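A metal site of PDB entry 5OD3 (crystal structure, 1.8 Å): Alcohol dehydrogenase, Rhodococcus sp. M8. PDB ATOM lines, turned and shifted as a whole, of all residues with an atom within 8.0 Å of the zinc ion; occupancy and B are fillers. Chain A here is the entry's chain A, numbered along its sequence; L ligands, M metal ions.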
ATOM      1  N   GLY A  36     -24.371   8.423 -19.470  1.00  0.00           N
ATOM      2  CA  GLY A  36     -23.802   8.027 -20.739  1.00  0.00           C
ATOM      3  C   GLY A  36     -23.091   9.181 -21.453  1.00  0.00           C
ATOM      4  O   GLY A  36     -23.510  10.326 -21.337  1.00  0.00           O
ATOM      5  N   LEU A  37     -22.008   8.867 -22.141  1.00  0.00           N
ATOM      6  CA  LEU A  37     -21.333   9.807 -23.050  1.00  0.00           C
ATOM      7  C   LEU A  37     -21.872   9.607 -24.445  1.00  0.00           C
ATOM      8  O   LEU A  37     -21.959   8.477 -24.908  1.00  0.00           O
ATOM      9  CB  LEU A  37     -19.844   9.515 -23.130  1.00  0.00           C
ATOM     10  CG  LEU A  37     -18.938   9.865 -21.961  1.00  0.00           C
ATOM     11  CD1 LEU A  37     -19.034   8.823 -20.867  1.00  0.00           C
ATOM     12  CD2 LEU A  37     -17.503   9.941 -22.509  1.00  0.00           C
ATOM     13  N   CYS A  38     -22.151  10.702 -25.140  1.00  0.00           N
ATOM     14  CA  CYS A  38     -22.724  10.641 -26.471  1.00  0.00           C
ATOM     15  C   CYS A  38     -21.909  11.505 -27.418  1.00  0.00           C
ATOM     16  O   CYS A  38     -21.407  12.550 -27.027  1.00  0.00           O
ATOM     17  CB  CYS A  38     -24.158  11.160 -26.421  1.00  0.00           C
ATOM     18  SG  CYS A  38     -24.991  11.233 -28.024  1.00  0.00           S
ATOM     19  N   HIS A  39     -21.836  11.101 -28.675  1.00  0.00           N
ATOM     20  CA  HIS A  39     -21.064  11.884 -29.639  1.00  0.00           C
ATOM     21  C   HIS A  39     -21.680  13.281 -29.857  1.00  0.00           C
ATOM     22  O   HIS A  39     -20.981  14.210 -30.257  1.00  0.00           O
ATOM     23  CB  HIS A  39     -20.891  11.146 -30.949  1.00  0.00           C
ATOM     24  CG  HIS A  39     -19.661  11.548 -31.693  1.00  0.00           C
ATOM     25  ND1 HIS A  39     -18.491  10.824 -31.629  1.00  0.00           N
ATOM     26  CD2 HIS A  39     -19.404  12.619 -32.481  1.00  0.00           C
ATOM     27  CE1 HIS A  39     -17.567  11.430 -32.370  1.00  0.00           C
ATOM     28  NE2 HIS A  39     -18.102  12.516 -32.889  1.00  0.00           N
ATOM     29  N   SER A  40     -22.972  13.447 -29.544  1.00  0.00           N
ATOM     30  CA  SER A  40     -23.567  14.783 -29.543  1.00  0.00           C
ATOM     31  C   SER A  40     -22.878  15.771 -28.584  1.00  0.00           C
ATOM     32  O   SER A  40     -22.854  16.987 -28.844  1.00  0.00           O
ATOM     33  CB  SER A  40     -25.064  14.729 -29.244  1.00  0.00           C
ATOM     34  OG  SER A  40     -25.732  14.143 -30.349  1.00  0.00           O
ATOM     35  N   ASP A  41     -22.308  15.246 -27.497  1.00  0.00           N
ATOM     36  CA  ASP A  41     -21.532  16.065 -26.553  1.00  0.00           C
ATOM     37  C   ASP A  41     -20.274  16.650 -27.248  1.00  0.00           C
ATOM     38  O   ASP A  41     -19.921  17.806 -27.023  1.00  0.00           O
ATOM     39  CB  ASP A  41     -21.093  15.255 -25.339  1.00  0.00           C
ATOM     40  CG  ASP A  41     -22.272  14.688 -24.539  1.00  0.00           C
ATOM     41  OD1 ASP A  41     -23.333  15.320 -24.554  1.00  0.00           O
ATOM     42  OD2 ASP A  41     -22.125  13.626 -23.905  1.00  0.00           O
ATOM     43  N   GLY A  61     -23.930  15.671 -19.972  1.00  0.00           N
ATOM     44  CA  GLY A  61     -24.586  14.390 -19.755  1.00  0.00           C
ATOM     45  C   GLY A  61     -26.067  14.483 -19.952  1.00  0.00           C
ATOM     46  O   GLY A  61     -26.797  14.979 -19.090  1.00  0.00           O
ATOM     47  N   HIS A  62     -26.532  13.993 -21.088  1.00  0.00           N
ATOM     48  CA  HIS A  62     -27.977  13.971 -21.339  1.00  0.00           C
ATOM     49  C   HIS A  62     -28.539  12.541 -21.346  1.00  0.00           C
ATOM     50  O   HIS A  62     -29.707  12.357 -21.684  1.00  0.00           O
ATOM     51  CB  HIS A  62     -28.304  14.732 -22.600  1.00  0.00           C
ATOM     52  CG  HIS A  62     -27.563  14.249 -23.783  1.00  0.00           C
ATOM     53  ND1 HIS A  62     -26.377  14.802 -24.194  1.00  0.00           N
ATOM     54  CD2 HIS A  62     -27.819  13.220 -24.624  1.00  0.00           C
ATOM     55  CE1 HIS A  62     -25.941  14.148 -25.256  1.00  0.00           C
ATOM     56  NE2 HIS A  62     -26.793  13.185 -25.524  1.00  0.00           N
ATOM     57  N   GLU A  63     -27.710  11.568 -20.948  1.00  0.00           N
ATOM     58  CA  GLU A  63     -28.124  10.194 -20.738  1.00  0.00           C
ATOM     59  C   GLU A  63     -27.973   9.870 -19.254  1.00  0.00           C
ATOM     60  O   GLU A  63     -26.882   9.548 -18.812  1.00  0.00           O
ATOM     61  CB  GLU A  63     -27.219   9.235 -21.529  1.00  0.00           C
ATOM     62  CG  GLU A  63     -27.435   9.224 -23.010  1.00  0.00           C
ATOM     63  CD  GLU A  63     -26.776   8.044 -23.701  1.00  0.00           C
ATOM     64  OE1 GLU A  63     -25.810   7.431 -23.203  1.00  0.00           O
ATOM     65  OE2 GLU A  63     -27.227   7.712 -24.812  1.00  0.00           O
ATOM     66  N   THR A 152     -31.736   6.059 -22.602  1.00  0.00           N
ATOM     67  CA  THR A 152     -32.298   7.391 -22.664  1.00  0.00           C
ATOM     68  C   THR A 152     -31.971   8.194 -23.926  1.00  0.00           C
ATOM     69  O   THR A 152     -32.570   9.237 -24.137  1.00  0.00           O
ATOM     70  CB  THR A 152     -31.859   8.222 -21.422  1.00  0.00           C
ATOM     71  OG1 THR A 152     -30.435   8.314 -21.370  1.00  0.00           O
ATOM     72  CG2 THR A 152     -32.358   7.575 -20.179  1.00  0.00           C
ATOM     73  N   ASP A 153     -31.024   7.725 -24.726  1.00  0.00           N
ATOM     74  CA  ASP A 153     -30.656   8.418 -25.959  1.00  0.00           C
ATOM     75  C   ASP A 153     -30.150   7.441 -27.000  1.00  0.00           C
ATOM     76  O   ASP A 153     -30.711   7.363 -28.086  1.00  0.00           O
ATOM     77  CB  ASP A 153     -29.639   9.462 -25.617  1.00  0.00           C
ATOM     78  CG  ASP A 153     -29.352  10.423 -26.744  1.00  0.00           C
ATOM     79  OD1 ASP A 153     -30.162  10.618 -27.680  1.00  0.00           O
ATOM     80  OD2 ASP A 153     -28.275  11.012 -26.626  1.00  0.00           O
ATOM     81  N   ALA A 154     -29.126   6.647 -26.671  1.00  0.00           N
ATOM     82  CA  ALA A 154     -28.700   5.593 -27.574  1.00  0.00           C
ATOM     83  C   ALA A 154     -29.811   4.612 -27.885  1.00  0.00           C
ATOM     84  O   ALA A 154     -29.846   4.026 -28.963  1.00  0.00           O
ATOM     85  CB  ALA A 154     -27.462   4.864 -27.031  1.00  0.00           C
ATOM     86  N   THR A 157     -33.360   7.489 -29.250  1.00  0.00           N
ATOM     87  CA  THR A 157     -33.242   8.162 -30.554  1.00  0.00           C
ATOM     88  C   THR A 157     -33.420   7.195 -31.731  1.00  0.00           C
ATOM     89  O   THR A 157     -34.235   7.465 -32.612  1.00  0.00           O
ATOM     90  CB  THR A 157     -31.983   9.000 -30.608  1.00  0.00           C
ATOM     91  OG1 THR A 157     -32.077  10.023 -29.596  1.00  0.00           O
ATOM     92  CG2 THR A 157     -31.815   9.663 -31.959  1.00  0.00           C
ATOM     93  N   LEU A 183     -25.451   4.582 -30.623  1.00  0.00           N
ATOM     94  CA  LEU A 183     -26.815   4.542 -31.152  1.00  0.00           C
ATOM     95  C   LEU A 183     -26.994   3.339 -32.075  1.00  0.00           C
ATOM     96  O   LEU A 183     -27.956   2.582 -31.919  1.00  0.00           O
ATOM     97  CB  LEU A 183     -27.163   5.821 -31.921  1.00  0.00           C
ATOM     98  CG  LEU A 183     -27.800   6.932 -31.115  1.00  0.00           C
ATOM     99  CD1 LEU A 183     -26.857   7.535 -30.098  1.00  0.00           C
ATOM    100  CD2 LEU A 183     -28.314   8.038 -32.046  1.00  0.00           C
ATOM    101  N   ILE A 271     -25.150  13.634 -36.929  1.00  0.00           N
ATOM    102  CA  ILE A 271     -24.979  15.078 -37.151  1.00  0.00           C
ATOM    103  C   ILE A 271     -23.552  15.373 -37.611  1.00  0.00           C
ATOM    104  O   ILE A 271     -22.608  15.111 -36.872  1.00  0.00           O
ATOM    105  CB  ILE A 271     -25.282  15.909 -35.864  1.00  0.00           C
ATOM    106  CG1 ILE A 271     -26.657  15.532 -35.289  1.00  0.00           C
ATOM    107  CG2 ILE A 271     -25.294  17.401 -36.205  1.00  0.00           C
ATOM    108  CD1 ILE A 271     -26.979  16.051 -33.904  1.00  0.00           C
ATOM    109  N   TRP A 295     -34.282  12.999 -31.068  1.00  0.00           N
ATOM    110  CA  TRP A 295     -34.473  12.353 -29.766  1.00  0.00           C
ATOM    111  C   TRP A 295     -35.700  11.437 -29.812  1.00  0.00           C
ATOM    112  O   TRP A 295     -35.784  10.626 -30.754  1.00  0.00           O
ATOM    113  CB  TRP A 295     -34.458  13.403 -28.630  1.00  0.00           C
ATOM    114  CG  TRP A 295     -33.750  12.935 -27.414  1.00  0.00           C
ATOM    115  CD1 TRP A 295     -33.628  11.660 -26.961  1.00  0.00           C
ATOM    116  CD2 TRP A 295     -33.061  13.759 -26.454  1.00  0.00           C
ATOM    117  NE1 TRP A 295     -32.892  11.622 -25.795  1.00  0.00           N
ATOM    118  CE2 TRP A 295     -32.534  12.900 -25.462  1.00  0.00           C
ATOM    119  CE3 TRP A 295     -32.826  15.128 -26.371  1.00  0.00           C
ATOM    120  CZ2 TRP A 295     -31.801  13.380 -24.383  1.00  0.00           C
ATOM    121  CZ3 TRP A 295     -32.106  15.616 -25.275  1.00  0.00           C
ATOM    122  CH2 TRP A 295     -31.600  14.740 -24.309  1.00  0.00           C
ATOM    123  N   ARG A 340     -21.100   2.005 -25.873  1.00  0.00           N
ATOM    124  CA  ARG A 340     -21.343   3.257 -25.159  1.00  0.00           C
ATOM    125  C   ARG A 340     -20.423   3.412 -23.953  1.00  0.00           C
ATOM    126  O   ARG A 340     -20.305   2.490 -23.138  1.00  0.00           O
ATOM    127  CB  ARG A 340     -22.785   3.285 -24.630  1.00  0.00           C
ATOM    128  CG  ARG A 340     -23.676   4.253 -25.349  1.00  0.00           C
ATOM    129  CD  ARG A 340     -23.359   5.668 -24.974  1.00  0.00           C
ATOM    130  NE  ARG A 340     -24.370   6.605 -25.475  1.00  0.00           N
ATOM    131  CZ  ARG A 340     -24.344   7.227 -26.656  1.00  0.00           C
ATOM    132  NH1 ARG A 340     -23.377   7.014 -27.550  1.00  0.00           N
ATOM    133  NH2 ARG A 340     -25.316   8.084 -26.921  1.00  0.00           N
HETATM  134  P1  LIG L   1     -20.302   6.960 -31.683  1.00  0.00           P
HETATM  135  O1  LIG L   1     -19.069   7.776 -31.639  1.00  0.00           O
HETATM  136  O2  LIG L   1     -20.674   5.972 -30.589  1.00  0.00           O
HETATM  137  O3  LIG L   1     -20.348   6.093 -33.006  1.00  0.00           O
HETATM  138  C1  LIG L   1     -19.432   6.265 -34.045  1.00  0.00           C
HETATM  139  C2  LIG L   1     -19.494   5.028 -34.911  1.00  0.00           C
HETATM  140  O4  LIG L   1     -19.676   5.548 -36.219  1.00  0.00           O
HETATM  141  C3  LIG L   1     -18.208   4.211 -34.901  1.00  0.00           C
HETATM  142  O5  LIG L   1     -18.455   2.803 -34.933  1.00  0.00           O
HETATM  143  C4  LIG L   1     -17.518   4.641 -36.179  1.00  0.00           C
HETATM  144  O6  LIG L   1     -16.687   3.653 -36.760  1.00  0.00           O
HETATM  145  C5  LIG L   1     -18.731   4.913 -37.061  1.00  0.00           C
HETATM  146  N1  LIG L   1     -18.483   5.741 -38.232  1.00  0.00           N
HETATM  147  C6  LIG L   1     -17.853   6.944 -38.264  1.00  0.00           C
HETATM  148  N2  LIG L   1     -17.808   7.404 -39.533  1.00  0.00           N
HETATM  149  C7  LIG L   1     -18.385   6.474 -40.328  1.00  0.00           C
HETATM  150  C8  LIG L   1     -18.683   6.360 -41.732  1.00  0.00           C
HETATM  151  N3  LIG L   1     -18.284   7.345 -42.589  1.00  0.00           N
HETATM  152  N4  LIG L   1     -19.347   5.263 -42.166  1.00  0.00           N
HETATM  153  C9  LIG L   1     -19.729   4.287 -41.295  1.00  0.00           C
HETATM  154  N5  LIG L   1     -19.481   4.330 -39.985  1.00  0.00           N
HETATM  155  C10 LIG L   1     -18.817   5.383 -39.464  1.00  0.00           C
HETATM  156  O7  LIG L   1     -21.557   7.954 -31.987  1.00  0.00           O
HETATM  157  P2  LIG L   1     -22.995   7.950 -31.236  1.00  0.00           P
HETATM  158  O8  LIG L   1     -22.787   8.536 -29.837  1.00  0.00           O
HETATM  159  O9  LIG L   1     -23.635   6.587 -31.448  1.00  0.00           O
HETATM  160  O10 LIG L   1     -23.748   9.098 -32.062  1.00  0.00           O
HETATM  161  C11 LIG L   1     -24.016   8.887 -33.451  1.00  0.00           C
HETATM  162  C12 LIG L   1     -24.487  10.171 -34.100  1.00  0.00           C
HETATM  163  O11 LIG L   1     -25.842  10.410 -33.737  1.00  0.00           O
HETATM  164  C13 LIG L   1     -23.683  11.429 -33.750  1.00  0.00           C
HETATM  165  O12 LIG L   1     -23.549  12.202 -34.951  1.00  0.00           O
HETATM  166  C14 LIG L   1     -24.551  12.081 -32.720  1.00  0.00           C
HETATM  167  O13 LIG L   1     -24.279  13.481 -32.618  1.00  0.00           O
HETATM  168  C15 LIG L   1     -25.943  11.742 -33.248  1.00  0.00           C
HETATM  169  N6  LIG L   1     -27.093  11.830 -32.336  1.00  0.00           N
HETATM  170  C16 LIG L   1     -28.214  12.366 -32.843  1.00  0.00           C
HETATM  171  C17 LIG L   1     -29.373  12.497 -32.113  1.00  0.00           C
HETATM  172  C18 LIG L   1     -30.609  13.063 -32.739  1.00  0.00           C
HETATM  173  O14 LIG L   1     -31.526  13.423 -31.996  1.00  0.00           O
HETATM  174  N7  LIG L   1     -30.778  13.120 -34.085  1.00  0.00           N
HETATM  175  C19 LIG L   1     -29.375  12.042 -30.790  1.00  0.00           C
HETATM  176  C20 LIG L   1     -28.209  11.451 -30.277  1.00  0.00           C
HETATM  177  C21 LIG L   1     -27.074  11.365 -31.058  1.00  0.00           C
HETATM  178 ZN    ZN M   1     -26.929  12.218 -27.305  1.00  0.00          ZN
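N of Cys 38 sits at hydrogen-bond distance from OD2 of Asp 41, at 3.2 Å.
The side-chain sulfur of Cys 38 lies close to the backbone NH of Ser 40 (3.4 Å).
The side-chain sulfur (SG) of Cys 38 sits close to the guanidinium group (NH2) of Arg 340, at 3.4 Å.
The indole nitrogen (NE1) of Trp 295 lies within hydrogen-bond range of the side-chain carboxylate (OD1) of Asp 153 (3.5 Å).
OG1 of Thr 157 lies within hydrogen-bond range of OD1 of Asp 153.
A ring nitrogen (ND1) of His 62 sits close to the side-chain carboxylate (OD1) of Asp 41, at 3.1 Å.
The zinc ion is bound by OD2 of Asp 153.
The zinc ion is bound by NE2 of His 62 (2.0 Å).
The zinc ion is bound by SG of Cys 38 (2.3 Å).
Residues that only touch the zinc ion: Ser 40 (3.7 Å).
Of the 17 residues printed, 4 come within 4 Å of the zinc ion.
The backbone NH (N) of His 39 sits at hydrogen-bond distance from an oxygen (O8) of the ligand, at 3.0 Å.
An oxygen (O12) of the ligand is in hydrogen-bond range of the backbone NH (N) of Ile 271, at 2.9 Å.
The guanidinium group (NH1) of Arg 340 lies within salt-bridge range of an oxygen (O8) of the ligand (2.8 Å).
ND1 of His 39 is in hydrogen-bond range of O1 of the ligand (3.1 Å).
OG of Ser 40 lies within hydrogen-bond range of O13 of the ligand (2.8 Å).
An oxygen (O9) of the ligand is in hydrogen-bond range of the backbone NH (N) of Leu 183 (2.8 Å).
The backbone NH (N) of Trp 295 is in hydrogen-bond range of an oxygen (O14) of the ligand, 2.9 Å away.
N of Ser 40 sits at hydrogen-bond distance from O13 of the ligand, at 3.3 Å.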
